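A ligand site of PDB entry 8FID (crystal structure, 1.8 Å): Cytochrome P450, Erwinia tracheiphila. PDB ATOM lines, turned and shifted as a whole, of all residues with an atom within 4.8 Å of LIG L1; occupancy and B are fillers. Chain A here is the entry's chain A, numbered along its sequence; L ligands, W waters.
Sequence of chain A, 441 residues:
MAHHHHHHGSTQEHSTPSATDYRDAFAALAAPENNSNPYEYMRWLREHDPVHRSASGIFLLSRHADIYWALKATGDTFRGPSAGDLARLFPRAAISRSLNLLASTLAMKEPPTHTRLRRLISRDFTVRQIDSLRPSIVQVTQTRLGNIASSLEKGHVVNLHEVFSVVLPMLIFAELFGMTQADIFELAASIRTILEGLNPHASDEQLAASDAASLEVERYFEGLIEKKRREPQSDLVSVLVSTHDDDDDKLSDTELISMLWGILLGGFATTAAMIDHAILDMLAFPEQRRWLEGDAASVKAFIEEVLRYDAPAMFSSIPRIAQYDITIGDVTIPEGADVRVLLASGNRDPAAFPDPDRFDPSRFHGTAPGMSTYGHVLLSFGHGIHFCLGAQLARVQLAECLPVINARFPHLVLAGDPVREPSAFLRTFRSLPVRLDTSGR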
ATOM      1  N   LEU A  71       0.130  -1.512 -38.667  1.00  0.00           N
ATOM      2  CA  LEU A  71       1.047  -1.290 -37.555  1.00  0.00           C
ATOM      3  C   LEU A  71       2.341  -2.074 -37.737  1.00  0.00           C
ATOM      4  O   LEU A  71       3.438  -1.524 -37.561  1.00  0.00           O
ATOM      5  CB  LEU A  71       0.341  -1.660 -36.238  1.00  0.00           C
ATOM      6  CG  LEU A  71      -0.844  -0.790 -35.853  1.00  0.00           C
ATOM      7  CD1 LEU A  71      -1.725  -1.482 -34.818  1.00  0.00           C
ATOM      8  CD2 LEU A  71      -0.362   0.561 -35.303  1.00  0.00           C
ATOM      9  N   LEU A 106       9.696  10.455 -31.694  1.00  0.00           N
ATOM     10  CA  LEU A 106      10.146   9.181 -32.234  1.00  0.00           C
ATOM     11  C   LEU A 106       9.019   8.392 -32.883  1.00  0.00           C
ATOM     12  O   LEU A 106       9.302   7.483 -33.680  1.00  0.00           O
ATOM     13  CB  LEU A 106      10.787   8.345 -31.134  1.00  0.00           C
ATOM     14  CG  LEU A 106       9.871   7.601 -30.142  1.00  0.00           C
ATOM     15  CD1 LEU A 106      10.725   6.627 -29.339  1.00  0.00           C
ATOM     16  CD2 LEU A 106       9.132   8.547 -29.223  1.00  0.00           C
ATOM     17  N   ALA A 107       7.768   8.712 -32.576  1.00  0.00           N
ATOM     18  CA  ALA A 107       6.636   8.015 -33.186  1.00  0.00           C
ATOM     19  C   ALA A 107       6.524   8.310 -34.681  1.00  0.00           C
ATOM     20  O   ALA A 107       5.827   7.575 -35.392  1.00  0.00           O
ATOM     21  CB  ALA A 107       5.344   8.400 -32.478  1.00  0.00           C
ATOM     22  N   HIS A 114      14.634   5.920 -35.218  1.00  0.00           N
ATOM     23  CA  HIS A 114      13.709   5.461 -34.188  1.00  0.00           C
ATOM     24  C   HIS A 114      14.423   4.628 -33.133  1.00  0.00           C
ATOM     25  O   HIS A 114      14.145   4.763 -31.936  1.00  0.00           O
ATOM     26  CB  HIS A 114      12.573   4.643 -34.810  1.00  0.00           C
ATOM     27  CG  HIS A 114      11.664   4.041 -33.795  1.00  0.00           C
ATOM     28  ND1 HIS A 114      11.798   2.747 -33.341  1.00  0.00           N
ATOM     29  CD2 HIS A 114      10.605   4.569 -33.117  1.00  0.00           C
ATOM     30  CE1 HIS A 114      10.851   2.492 -32.452  1.00  0.00           C
ATOM     31  NE2 HIS A 114      10.121   3.586 -32.285  1.00  0.00           N
ATOM     32  N   ARG A 118      14.488   5.573 -29.144  1.00  0.00           N
ATOM     33  CA  ARG A 118      13.817   4.706 -28.198  1.00  0.00           C
ATOM     34  C   ARG A 118      14.786   4.173 -27.140  1.00  0.00           C
ATOM     35  O   ARG A 118      14.424   4.037 -25.963  1.00  0.00           O
ATOM     36  CB  ARG A 118      13.135   3.543 -28.920  1.00  0.00           C
ATOM     37  CG  ARG A 118      12.407   2.579 -27.990  1.00  0.00           C
ATOM     38  CD  ARG A 118      11.136   2.033 -28.618  1.00  0.00           C
ATOM     39  NE  ARG A 118      10.444   1.110 -27.727  1.00  0.00           N
ATOM     40  CZ  ARG A 118       9.135   0.900 -27.738  1.00  0.00           C
ATOM     41  NH1 ARG A 118       8.338   1.552 -28.574  1.00  0.00           N
ATOM     42  NH2 ARG A 118       8.606   0.026 -26.882  1.00  0.00           N
ATOM     43  N   ILE A 121      15.326   6.153 -23.897  1.00  0.00           N
ATOM     44  CA  ILE A 121      14.241   6.289 -22.943  1.00  0.00           C
ATOM     45  C   ILE A 121      13.697   4.962 -22.441  1.00  0.00           C
ATOM     46  O   ILE A 121      12.870   4.969 -21.515  1.00  0.00           O
ATOM     47  CB  ILE A 121      13.089   7.135 -23.518  1.00  0.00           C
ATOM     48  CG1 ILE A 121      12.531   6.480 -24.784  1.00  0.00           C
ATOM     49  CG2 ILE A 121      13.557   8.550 -23.826  1.00  0.00           C
ATOM     50  CD1 ILE A 121      11.283   7.140 -25.320  1.00  0.00           C
ATOM     51  N   PHE A 125      11.185   2.241 -18.489  1.00  0.00           N
ATOM     52  CA  PHE A 125       9.883   1.636 -18.718  1.00  0.00           C
ATOM     53  C   PHE A 125       9.947   0.117 -18.805  1.00  0.00           C
ATOM     54  O   PHE A 125       8.937  -0.521 -19.125  1.00  0.00           O
ATOM     55  CB  PHE A 125       9.261   2.207 -20.005  1.00  0.00           C
ATOM     56  CG  PHE A 125       8.975   3.688 -19.909  1.00  0.00           C
ATOM     57  CD1 PHE A 125       7.790   4.149 -19.371  1.00  0.00           C
ATOM     58  CD2 PHE A 125       9.913   4.616 -20.352  1.00  0.00           C
ATOM     59  CE1 PHE A 125       7.530   5.489 -19.280  1.00  0.00           C
ATOM     60  CE2 PHE A 125       9.659   5.969 -20.260  1.00  0.00           C
ATOM     61  CZ  PHE A 125       8.472   6.407 -19.724  1.00  0.00           C
ATOM     62  N   PHE A 173       4.000   9.360 -12.996  1.00  0.00           N
ATOM     63  CA  PHE A 173       4.749   9.816 -14.156  1.00  0.00           C
ATOM     64  C   PHE A 173       5.741  10.918 -13.771  1.00  0.00           C
ATOM     65  O   PHE A 173       6.898  10.899 -14.185  1.00  0.00           O
ATOM     66  CB  PHE A 173       3.821  10.327 -15.249  1.00  0.00           C
ATOM     67  CG  PHE A 173       4.538  10.994 -16.377  1.00  0.00           C
ATOM     68  CD1 PHE A 173       5.118  10.244 -17.389  1.00  0.00           C
ATOM     69  CD2 PHE A 173       4.681  12.373 -16.408  1.00  0.00           C
ATOM     70  CE1 PHE A 173       5.806  10.855 -18.410  1.00  0.00           C
ATOM     71  CE2 PHE A 173       5.379  12.987 -17.419  1.00  0.00           C
ATOM     72  CZ  PHE A 173       5.941  12.229 -18.430  1.00  0.00           C
ATOM     73  N   ILE A 263       6.522  12.754 -24.503  1.00  0.00           N
ATOM     74  CA  ILE A 263       6.353  11.862 -23.349  1.00  0.00           C
ATOM     75  C   ILE A 263       5.351  12.454 -22.367  1.00  0.00           C
ATOM     76  O   ILE A 263       4.535  11.734 -21.782  1.00  0.00           O
ATOM     77  CB  ILE A 263       7.710  11.601 -22.681  1.00  0.00           C
ATOM     78  CG1 ILE A 263       8.695  10.946 -23.648  1.00  0.00           C
ATOM     79  CG2 ILE A 263       7.529  10.716 -21.445  1.00  0.00           C
ATOM     80  CD1 ILE A 263       8.294   9.562 -24.096  1.00  0.00           C
ATOM     81  N   GLY A 266       1.857  11.729 -23.592  1.00  0.00           N
ATOM     82  CA  GLY A 266       1.470  10.344 -23.427  1.00  0.00           C
ATOM     83  C   GLY A 266       1.537   9.812 -22.021  1.00  0.00           C
ATOM     84  O   GLY A 266       1.124   8.677 -21.771  1.00  0.00           O
ATOM     85  N   GLY A 267       2.012  10.623 -21.069  1.00  0.00           N
ATOM     86  CA  GLY A 267       2.433  10.120 -19.773  1.00  0.00           C
ATOM     87  C   GLY A 267       1.333   9.770 -18.803  1.00  0.00           C
ATOM     88  O   GLY A 267       1.588   8.992 -17.875  1.00  0.00           O
ATOM     89  N   THR A 270      -4.025   8.996 -21.026  1.00  0.00           N
ATOM     90  CA  THR A 270      -4.639   7.738 -21.439  1.00  0.00           C
ATOM     91  C   THR A 270      -4.673   6.729 -20.294  1.00  0.00           C
ATOM     92  O   THR A 270      -5.608   5.932 -20.211  1.00  0.00           O
ATOM     93  CB  THR A 270      -3.879   7.146 -22.617  1.00  0.00           C
ATOM     94  OG1 THR A 270      -2.467   7.252 -22.371  1.00  0.00           O
ATOM     95  CG2 THR A 270      -4.239   7.870 -23.916  1.00  0.00           C
ATOM     96  N   THR A 271      -3.661   6.736 -19.419  1.00  0.00           N
ATOM     97  CA  THR A 271      -3.697   5.864 -18.251  1.00  0.00           C
ATOM     98  C   THR A 271      -4.875   6.221 -17.361  1.00  0.00           C
ATOM     99  O   THR A 271      -5.611   5.330 -16.896  1.00  0.00           O
ATOM    100  CB  THR A 271      -2.383   5.975 -17.475  1.00  0.00           C
ATOM    101  OG1 THR A 271      -1.292   5.645 -18.337  1.00  0.00           O
ATOM    102  CG2 THR A 271      -2.391   5.036 -16.285  1.00  0.00           C
ATOM    103  N   MET A 274      -7.965   4.821 -18.834  1.00  0.00           N
ATOM    104  CA  MET A 274      -8.037   3.389 -18.561  1.00  0.00           C
ATOM    105  C   MET A 274      -8.568   3.123 -17.156  1.00  0.00           C
ATOM    106  O   MET A 274      -9.419   2.260 -16.953  1.00  0.00           O
ATOM    107  CB  MET A 274      -6.662   2.748 -18.756  1.00  0.00           C
ATOM    108  CG  MET A 274      -6.619   1.241 -18.558  1.00  0.00           C
ATOM    109  SD  MET A 274      -4.920   0.592 -18.480  1.00  0.00           S
ATOM    110  CE  MET A 274      -4.319   1.391 -16.993  1.00  0.00           C
ATOM    111  N   LEU A 307      -8.949  -2.806 -21.483  1.00  0.00           N
ATOM    112  CA  LEU A 307      -8.245  -2.158 -22.572  1.00  0.00           C
ATOM    113  C   LEU A 307      -8.860  -2.522 -23.927  1.00  0.00           C
ATOM    114  O   LEU A 307      -8.951  -1.670 -24.817  1.00  0.00           O
ATOM    115  CB  LEU A 307      -6.770  -2.557 -22.538  1.00  0.00           C
ATOM    116  CG  LEU A 307      -5.911  -1.804 -21.513  1.00  0.00           C
ATOM    117  CD1 LEU A 307      -4.643  -2.603 -21.202  1.00  0.00           C
ATOM    118  CD2 LEU A 307      -5.576  -0.418 -22.037  1.00  0.00           C
ATOM    119  N   PRO A 312      -8.512   3.683 -24.784  1.00  0.00           N
ATOM    120  CA  PRO A 312      -8.467   5.134 -24.479  1.00  0.00           C
ATOM    121  C   PRO A 312      -8.336   6.009 -25.713  1.00  0.00           C
ATOM    122  O   PRO A 312      -8.918   7.101 -25.746  1.00  0.00           O
ATOM    123  CB  PRO A 312      -7.245   5.265 -23.555  1.00  0.00           C
ATOM    124  CG  PRO A 312      -7.086   3.919 -22.937  1.00  0.00           C
ATOM    125  CD  PRO A 312      -7.502   2.931 -24.020  1.00  0.00           C
ATOM    126  N   SER A 316      -5.003   6.692 -33.569  1.00  0.00           N
ATOM    127  CA  SER A 316      -3.784   7.376 -33.187  1.00  0.00           C
ATOM    128  C   SER A 316      -3.611   8.672 -33.971  1.00  0.00           C
ATOM    129  O   SER A 316      -3.909   8.725 -35.176  1.00  0.00           O
ATOM    130  CB  SER A 316      -2.562   6.479 -33.396  1.00  0.00           C
ATOM    131  OG  SER A 316      -1.376   7.163 -33.041  1.00  0.00           O
ATOM    132  N   ILE A 318      -0.899   9.680 -34.907  1.00  0.00           N
ATOM    133  CA  ILE A 318       0.328   9.526 -35.680  1.00  0.00           C
ATOM    134  C   ILE A 318      -0.027   9.181 -37.120  1.00  0.00           C
ATOM    135  O   ILE A 318      -0.668   8.153 -37.368  1.00  0.00           O
ATOM    136  CB  ILE A 318       1.241   8.447 -35.072  1.00  0.00           C
ATOM    137  CG1 ILE A 318       1.592   8.777 -33.613  1.00  0.00           C
ATOM    138  CG2 ILE A 318       2.500   8.292 -35.908  1.00  0.00           C
ATOM    139  CD1 ILE A 318       2.114  10.194 -33.391  1.00  0.00           C
ATOM    140  N   ARG A 320       0.508   7.666 -40.826  1.00  0.00           N
ATOM    141  CA  ARG A 320       1.280   6.652 -41.522  1.00  0.00           C
ATOM    142  C   ARG A 320       1.161   6.912 -43.020  1.00  0.00           C
ATOM    143  O   ARG A 320       0.050   6.848 -43.572  1.00  0.00           O
ATOM    144  CB  ARG A 320       0.811   5.241 -41.153  1.00  0.00           C
ATOM    145  CG  ARG A 320       1.297   4.820 -39.773  1.00  0.00           C
ATOM    146  CD  ARG A 320       0.679   3.514 -39.254  1.00  0.00           C
ATOM    147  NE  ARG A 320       1.442   3.039 -38.108  1.00  0.00           N
ATOM    148  CZ  ARG A 320       1.316   3.514 -36.868  1.00  0.00           C
ATOM    149  NH1 ARG A 320       0.412   4.459 -36.594  1.00  0.00           N
ATOM    150  NH2 ARG A 320       2.072   3.045 -35.892  1.00  0.00           N
ATOM    151  N   LEU A 343      -8.064   1.702 -33.832  1.00  0.00           N
ATOM    152  CA  LEU A 343      -7.744   0.693 -32.839  1.00  0.00           C
ATOM    153  C   LEU A 343      -8.997   0.172 -32.148  1.00  0.00           C
ATOM    154  O   LEU A 343      -9.172  -1.042 -31.960  1.00  0.00           O
ATOM    155  CB  LEU A 343      -6.777   1.262 -31.808  1.00  0.00           C
ATOM    156  CG  LEU A 343      -5.526   1.978 -32.320  1.00  0.00           C
ATOM    157  CD1 LEU A 343      -4.721   2.528 -31.140  1.00  0.00           C
ATOM    158  CD2 LEU A 343      -4.658   1.041 -33.145  1.00  0.00           C
ATOM    159  N   SER A 380      -5.057  -1.591 -28.397  1.00  0.00           N
ATOM    160  CA  SER A 380      -5.093  -0.292 -27.740  1.00  0.00           C
ATOM    161  C   SER A 380      -3.711   0.304 -27.516  1.00  0.00           C
ATOM    162  O   SER A 380      -3.597   1.528 -27.358  1.00  0.00           O
ATOM    163  CB  SER A 380      -5.824  -0.415 -26.399  1.00  0.00           C
ATOM    164  OG  SER A 380      -6.979  -1.242 -26.547  1.00  0.00           O
ATOM    165  N   PHE A 381      -2.657  -0.516 -27.496  1.00  0.00           N
ATOM    166  CA  PHE A 381      -1.292  -0.039 -27.343  1.00  0.00           C
ATOM    167  C   PHE A 381      -0.552   0.010 -28.672  1.00  0.00           C
ATOM    168  O   PHE A 381       0.665   0.208 -28.687  1.00  0.00           O
ATOM    169  CB  PHE A 381      -0.494  -0.924 -26.378  1.00  0.00           C
ATOM    170  CG  PHE A 381      -0.911  -0.832 -24.935  1.00  0.00           C
ATOM    171  CD1 PHE A 381      -0.881   0.385 -24.270  1.00  0.00           C
ATOM    172  CD2 PHE A 381      -1.285  -1.960 -24.244  1.00  0.00           C
ATOM    173  CE1 PHE A 381      -1.243   0.468 -22.932  1.00  0.00           C
ATOM    174  CE2 PHE A 381      -1.652  -1.890 -22.897  1.00  0.00           C
ATOM    175  CZ  PHE A 381      -1.632  -0.675 -22.251  1.00  0.00           C
ATOM    176  N   GLY A 382      -1.248  -0.198 -29.786  1.00  0.00           N
ATOM    177  CA  GLY A 382      -0.567  -0.289 -31.053  1.00  0.00           C
ATOM    178  C   GLY A 382       0.166  -1.624 -31.203  1.00  0.00           C
ATOM    179  O   GLY A 382      -0.116  -2.606 -30.504  1.00  0.00           O
ATOM    180  N   ILE A 385       6.924  -1.284 -34.490  1.00  0.00           N
ATOM    181  CA  ILE A 385       8.051  -0.526 -33.944  1.00  0.00           C
ATOM    182  C   ILE A 385       7.572   0.529 -32.950  1.00  0.00           C
ATOM    183  O   ILE A 385       8.321   0.913 -32.034  1.00  0.00           O
ATOM    184  CB  ILE A 385       8.897   0.117 -35.062  1.00  0.00           C
ATOM    185  CG1 ILE A 385       8.091   1.162 -35.840  1.00  0.00           C
ATOM    186  CG2 ILE A 385       9.459  -0.952 -36.012  1.00  0.00           C
ATOM    187  CD1 ILE A 385       8.957   1.973 -36.833  1.00  0.00           C
ATOM    188  N   HIS A 386       6.341   1.010 -33.102  1.00  0.00           N
ATOM    189  CA  HIS A 386       5.812   2.048 -32.228  1.00  0.00           C
ATOM    190  C   HIS A 386       4.908   1.491 -31.128  1.00  0.00           C
ATOM    191  O   HIS A 386       4.081   2.239 -30.585  1.00  0.00           O
ATOM    192  CB  HIS A 386       5.043   3.079 -33.040  1.00  0.00           C
ATOM    193  CG  HIS A 386       5.877   3.782 -34.061  1.00  0.00           C
ATOM    194  ND1 HIS A 386       7.062   4.416 -33.742  1.00  0.00           N
ATOM    195  CD2 HIS A 386       5.710   3.959 -35.393  1.00  0.00           C
ATOM    196  CE1 HIS A 386       7.574   4.952 -34.829  1.00  0.00           C
ATOM    197  NE2 HIS A 386       6.772   4.690 -35.852  1.00  0.00           N
ATOM    198  N   PHE A 387       5.045   0.211 -30.774  1.00  0.00           N
ATOM    199  CA  PHE A 387       4.268  -0.338 -29.671  1.00  0.00           C
ATOM    200  C   PHE A 387       4.518   0.485 -28.402  1.00  0.00           C
ATOM    201  O   PHE A 387       5.651   0.800 -28.059  1.00  0.00           O
ATOM    202  CB  PHE A 387       4.618  -1.800 -29.427  1.00  0.00           C
ATOM    203  CG  PHE A 387       3.878  -2.407 -28.252  1.00  0.00           C
ATOM    204  CD1 PHE A 387       2.623  -2.968 -28.420  1.00  0.00           C
ATOM    205  CD2 PHE A 387       4.441  -2.392 -26.977  1.00  0.00           C
ATOM    206  CE1 PHE A 387       1.933  -3.520 -27.353  1.00  0.00           C
ATOM    207  CE2 PHE A 387       3.747  -2.935 -25.909  1.00  0.00           C
ATOM    208  CZ  PHE A 387       2.505  -3.500 -26.088  1.00  0.00           C
ATOM    209  N   CYS A 388       3.427   0.780 -27.704  1.00  0.00           N
ATOM    210  CA  CYS A 388       3.464   1.693 -26.564  1.00  0.00           C
ATOM    211  C   CYS A 388       4.609   1.407 -25.604  1.00  0.00           C
ATOM    212  O   CYS A 388       4.764   0.301 -25.093  1.00  0.00           O
ATOM    213  CB  CYS A 388       2.133   1.601 -25.818  1.00  0.00           C
ATOM    214  SG  CYS A 388       2.146   2.489 -24.276  1.00  0.00           S
ATOM    215  N   LEU A 389       5.405   2.455 -25.353  1.00  0.00           N
ATOM    216  CA  LEU A 389       6.501   2.367 -24.391  1.00  0.00           C
ATOM    217  C   LEU A 389       5.993   2.206 -22.966  1.00  0.00           C
ATOM    218  O   LEU A 389       6.658   1.586 -22.129  1.00  0.00           O
ATOM    219  CB  LEU A 389       7.381   3.610 -24.489  1.00  0.00           C
ATOM    220  CG  LEU A 389       8.634   3.663 -23.624  1.00  0.00           C
ATOM    221  CD1 LEU A 389       9.640   2.619 -24.075  1.00  0.00           C
ATOM    222  CD2 LEU A 389       9.232   5.067 -23.659  1.00  0.00           C
ATOM    223  N   GLY A 390       4.831   2.780 -22.661  1.00  0.00           N
ATOM    224  CA  GLY A 390       4.327   2.815 -21.309  1.00  0.00           C
ATOM    225  C   GLY A 390       3.337   1.722 -20.939  1.00  0.00           C
ATOM    226  O   GLY A 390       2.740   1.783 -19.860  1.00  0.00           O
ATOM    227  N   LEU A 393       3.914   0.246 -17.510  1.00  0.00           N
ATOM    228  CA  LEU A 393       3.654   1.269 -16.493  1.00  0.00           C
ATOM    229  C   LEU A 393       2.153   1.454 -16.283  1.00  0.00           C
ATOM    230  O   LEU A 393       1.683   1.527 -15.141  1.00  0.00           O
ATOM    231  CB  LEU A 393       4.316   2.579 -16.893  1.00  0.00           C
ATOM    232  CG  LEU A 393       3.917   3.821 -16.098  1.00  0.00           C
ATOM    233  CD1 LEU A 393       4.173   3.596 -14.605  1.00  0.00           C
ATOM    234  CD2 LEU A 393       4.685   5.053 -16.582  1.00  0.00           C
ATOM    235  N   ALA A 394       1.388   1.519 -17.368  1.00  0.00           N
ATOM    236  CA  ALA A 394      -0.056   1.641 -17.259  1.00  0.00           C
ATOM    237  C   ALA A 394      -0.675   0.398 -16.623  1.00  0.00           C
ATOM    238  O   ALA A 394      -1.467   0.504 -15.680  1.00  0.00           O
ATOM    239  CB  ALA A 394      -0.675   1.888 -18.637  1.00  0.00           C
HETATM  240  C1  LIG L   1       2.925   4.686 -28.263  1.00  0.00           C
HETATM  241  C2  LIG L   1      -1.491   4.132 -26.336  1.00  0.00           C
HETATM  242  C3  LIG L   1       0.337   5.023 -21.926  1.00  0.00           C
HETATM  243  C4  LIG L   1       4.473   6.480 -24.002  1.00  0.00           C
HETATM  244  C5  LIG L   1       1.581   4.434 -28.134  1.00  0.00           C
HETATM  245  C6  LIG L   1       0.652   4.059 -29.200  1.00  0.00           C
HETATM  246  C7  LIG L   1      -0.553   3.914 -28.667  1.00  0.00           C
HETATM  247  C8  LIG L   1      -0.457   4.175 -27.240  1.00  0.00           C
HETATM  248  C9  LIG L   1      -1.848   3.500 -29.392  1.00  0.00           C
HETATM  249  C10 LIG L   1       1.033   3.847 -30.672  1.00  0.00           C
HETATM  250  C11 LIG L   1       0.550   5.021 -31.518  1.00  0.00           C
HETATM  251  C12 LIG L   1       0.798   4.710 -32.981  1.00  0.00           C
HETATM  252  O1  LIG L   1       1.495   3.716 -33.278  1.00  0.00           O
HETATM  253  O2  LIG L   1       0.299   5.478 -33.845  1.00  0.00           O
HETATM  254  C13 LIG L   1      -1.364   4.239 -24.965  1.00  0.00           C
HETATM  255  C14 LIG L   1      -2.362   3.876 -23.992  1.00  0.00           C
HETATM  256  C15 LIG L   1      -1.861   4.143 -22.770  1.00  0.00           C
HETATM  257  C16 LIG L   1      -0.516   4.652 -22.945  1.00  0.00           C
HETATM  258  C17 LIG L   1      -3.762   3.319 -24.332  1.00  0.00           C
HETATM  259  C18 LIG L   1      -2.488   3.927 -21.374  1.00  0.00           C
HETATM  260  C19 LIG L   1      -3.428   2.993 -21.163  1.00  0.00           C
HETATM  261  C20 LIG L   1       1.604   5.509 -22.098  1.00  0.00           C
HETATM  262  C21 LIG L   1       2.485   5.975 -21.051  1.00  0.00           C
HETATM  263  C22 LIG L   1       3.631   6.392 -21.605  1.00  0.00           C
HETATM  264  C23 LIG L   1       3.529   6.196 -23.046  1.00  0.00           C
HETATM  265  C24 LIG L   1       2.122   5.963 -19.551  1.00  0.00           C
HETATM  266  C25 LIG L   1       4.814   6.953 -20.769  1.00  0.00           C
HETATM  267  C26 LIG L   1       5.872   7.531 -21.332  1.00  0.00           C
HETATM  268  C27 LIG L   1       4.421   6.117 -25.341  1.00  0.00           C
HETATM  269  C28 LIG L   1       5.461   6.324 -26.321  1.00  0.00           C
HETATM  270  C29 LIG L   1       5.042   5.835 -27.498  1.00  0.00           C
HETATM  271  C30 LIG L   1       3.718   5.279 -27.309  1.00  0.00           C
HETATM  272  C31 LIG L   1       6.818   7.011 -26.037  1.00  0.00           C
HETATM  273  C32 LIG L   1       5.844   5.842 -28.814  1.00  0.00           C
HETATM  274  C33 LIG L   1       6.729   4.615 -28.883  1.00  0.00           C
HETATM  275  C34 LIG L   1       7.517   4.604 -30.179  1.00  0.00           C
HETATM  276  O3  LIG L   1       7.185   5.383 -31.112  1.00  0.00           O
HETATM  277  O4  LIG L   1       8.483   3.806 -30.283  1.00  0.00           O
HETATM  278  N1  LIG L   1       0.856   4.497 -26.967  1.00  0.00           N
HETATM  279  N2  LIG L   1      -0.239   4.720 -24.304  1.00  0.00           N
HETATM  280  N3  LIG L   1       2.274   5.657 -23.312  1.00  0.00           N
HETATM  281  N4  LIG L   1       3.379   5.461 -25.984  1.00  0.00           N
HETATM  282 FE1  LIG L   1       1.635   4.755 -25.068  1.00  0.00          FE
HETATM  283  C1  LG2 L   2       2.703   9.534 -27.904  1.00  0.00           C
HETATM  284  C2  LG2 L   2       3.619  11.819 -29.416  1.00  0.00           C
HETATM  285  C3  LG2 L   2       3.386   9.379 -29.269  1.00  0.00           C
HETATM  286  C4  LG2 L   2       6.218  10.738 -27.532  1.00  0.00           C
HETATM  287  C5  LG2 L   2      -1.959   8.580 -29.965  1.00  0.00           C
HETATM  288  C6  LG2 L   2      -0.608  11.666 -28.097  1.00  0.00           C
HETATM  289  C7  LG2 L   2      -2.061  11.414 -28.535  1.00  0.00           C
HETATM  290  C8  LG2 L   2      -2.593  10.087 -27.993  1.00  0.00           C
HETATM  291  C9  LG2 L   2      -1.745   8.901 -28.438  1.00  0.00           C
HETATM  292  C10 LG2 L   2      -0.305   9.187 -27.976  1.00  0.00           C
HETATM  293  C11 LG2 L   2       0.668   8.050 -28.222  1.00  0.00           C
HETATM  294  C12 LG2 L   2       1.981   8.264 -27.497  1.00  0.00           C
HETATM  295  C13 LG2 L   2       1.743  10.757 -27.882  1.00  0.00           C
HETATM  296  C14 LG2 L   2       2.465  12.019 -28.411  1.00  0.00           C
HETATM  297  C15 LG2 L   2       4.389  10.516 -29.243  1.00  0.00           C
HETATM  298  C16 LG2 L   2       4.976  10.398 -27.871  1.00  0.00           C
HETATM  299  C17 LG2 L   2       3.925   9.795 -26.978  1.00  0.00           C
HETATM  300  C18 LG2 L   2      -2.279   7.693 -27.724  1.00  0.00           C
HETATM  301  C19 LG2 L   2       0.431  10.518 -30.039  1.00  0.00           C
HETATM  302  C20 LG2 L   2       0.330  10.527 -28.542  1.00  0.00           C
HETATM  303  O1  LG2 L   2      -1.178   7.760 -30.522  1.00  0.00           O
HETATM  304  O2  LG2 L   2      -2.899   9.146 -30.559  1.00  0.00           O
HETATM  305  O   HOH W   1      -0.440   7.759 -24.026  1.00  0.00           O
HETATM  306  O   HOH W   2       2.127   1.141 -32.763  1.00  0.00           O
HETATM  307  O   HOH W   3      -1.022   7.624 -20.049  1.00  0.00           O
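Water W2 bridges an oxygen (O1) of LIG L1 and the backbone carbonyl oxygen of His 386. Water W1 bridges the side-chain hydroxyl of Thr 270 (2.7 Å) and the backbone carbonyl oxygen of Gly 266 (2.9 Å). Water W3 lies within hydrogen-bond range of the side-chain hydroxyl of Thr 271 (2.6 Å), the side-chain hydroxyl of Thr 270 (2.8 Å) and the backbone carbonyl oxygen of Gly 266 (2.9 Å).
The side-chain sulfur (SG) of Cys 388 sits close to the backbone NH (N) of Gly 390 (3.1 Å). A ring nitrogen (NE2) of His 386 lies within hydrogen-bond range of the backbone carbonyl oxygen of Ala 107. A ring nitrogen (NE2) of His 114 lies close to the backbone carbonyl oxygen (O) of Ile 385 (3.2 Å). ND1 of His 386 sits at hydrogen-bond distance from NE2 of His 114. The side-chain hydroxyl of Ser 380 sits at hydrogen-bond distance from the backbone carbonyl oxygen of Leu 307 (2.7 Å). The side-chain hydroxyl (OG) of Ser 316 lies close to the backbone NH (N) of Ile 318 (3.2 Å). The backbone NH of Cys 388 sits at hydrogen-bond distance from the backbone carbonyl oxygen of Phe 381 (3.0 Å). O of Phe 387 sits at hydrogen-bond distance from NH1 of Arg 118, 2.8 Å away.
O4 of LIG L1 sits close to O of Ile 385, at 3.4 Å. Leu 106 touches LIG L1 (CG to O3, 3.6 Å). Ala 107 touches LIG L1. CZ of Phe 125 touches C26 of LIG L1, at 3.3 Å. CD1 of Ile 263 touches C31 of LIG L1 (3.5 Å). O of Gly 266 touches C21 of LIG L1, 3.1 Å away. Gly 267 touches LIG L1 (O to C24, 3.5 Å). OG1 of Thr 270 touches C15 of LIG L1, at 3.2 Å. N of Thr 271 touches C18 of LIG L1, at 3.6 Å. Met 274 touches LIG L1. Pro 312 touches LIG L1 (CG to C17, 3.7 Å). Ile 318 touches LIG L1 (CB to O2, 3.3 Å). Leu 343 touches LIG L1 (CD1 to C9, 3.5 Å). Ser 380 touches LIG L1 (O to C9, 3.3 Å). Phe 381 touches LIG L1. Gly 382 touches LIG L1 (N to C9, 3.8 Å). N of Leu 389 touches N4 of LIG L1 (3.7 Å). Gly 390 touches LIG L1. Ala 394 touches LIG L1. Hydrophobic or aromatic side chains that line LIG L1: Leu 106, Ala 107, His 114, Phe 125, Ile 263, Met 274, Pro 312, Ile 318, Leu 343, Phe 381, His 386, Leu 389 and Ala 394. The nearest printed residue that does not touch LIG L1 is Leu 393 (4.03 Å).
The side-chain hydroxyl (OG) of Ser 316 is in hydrogen-bond range of an oxygen (O1) of LG2 L2 (2.6 Å). O4 of LIG L1 lies within salt-bridge range of NH1 of Arg 118, at 2.8 Å. O3 of LIG L1 sits at hydrogen-bond distance from ND1 of His 386, 2.8 Å away. The side-chain hydroxyl of Ser 316 sits at hydrogen-bond distance from an oxygen (O2) of LIG L1, 2.5 Å away. The guanidinium group of Arg 320 is in salt-bridge range of an oxygen (O1) of LIG L1 (2.8 Å). The side-chain sulfur (SG) of Cys 388 binds an iron atom (FE1) of LIG L1, 2.5 Å away. An oxygen (O4) of LIG L1 is in hydrogen-bond range of a ring nitrogen (NE2) of His 114.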
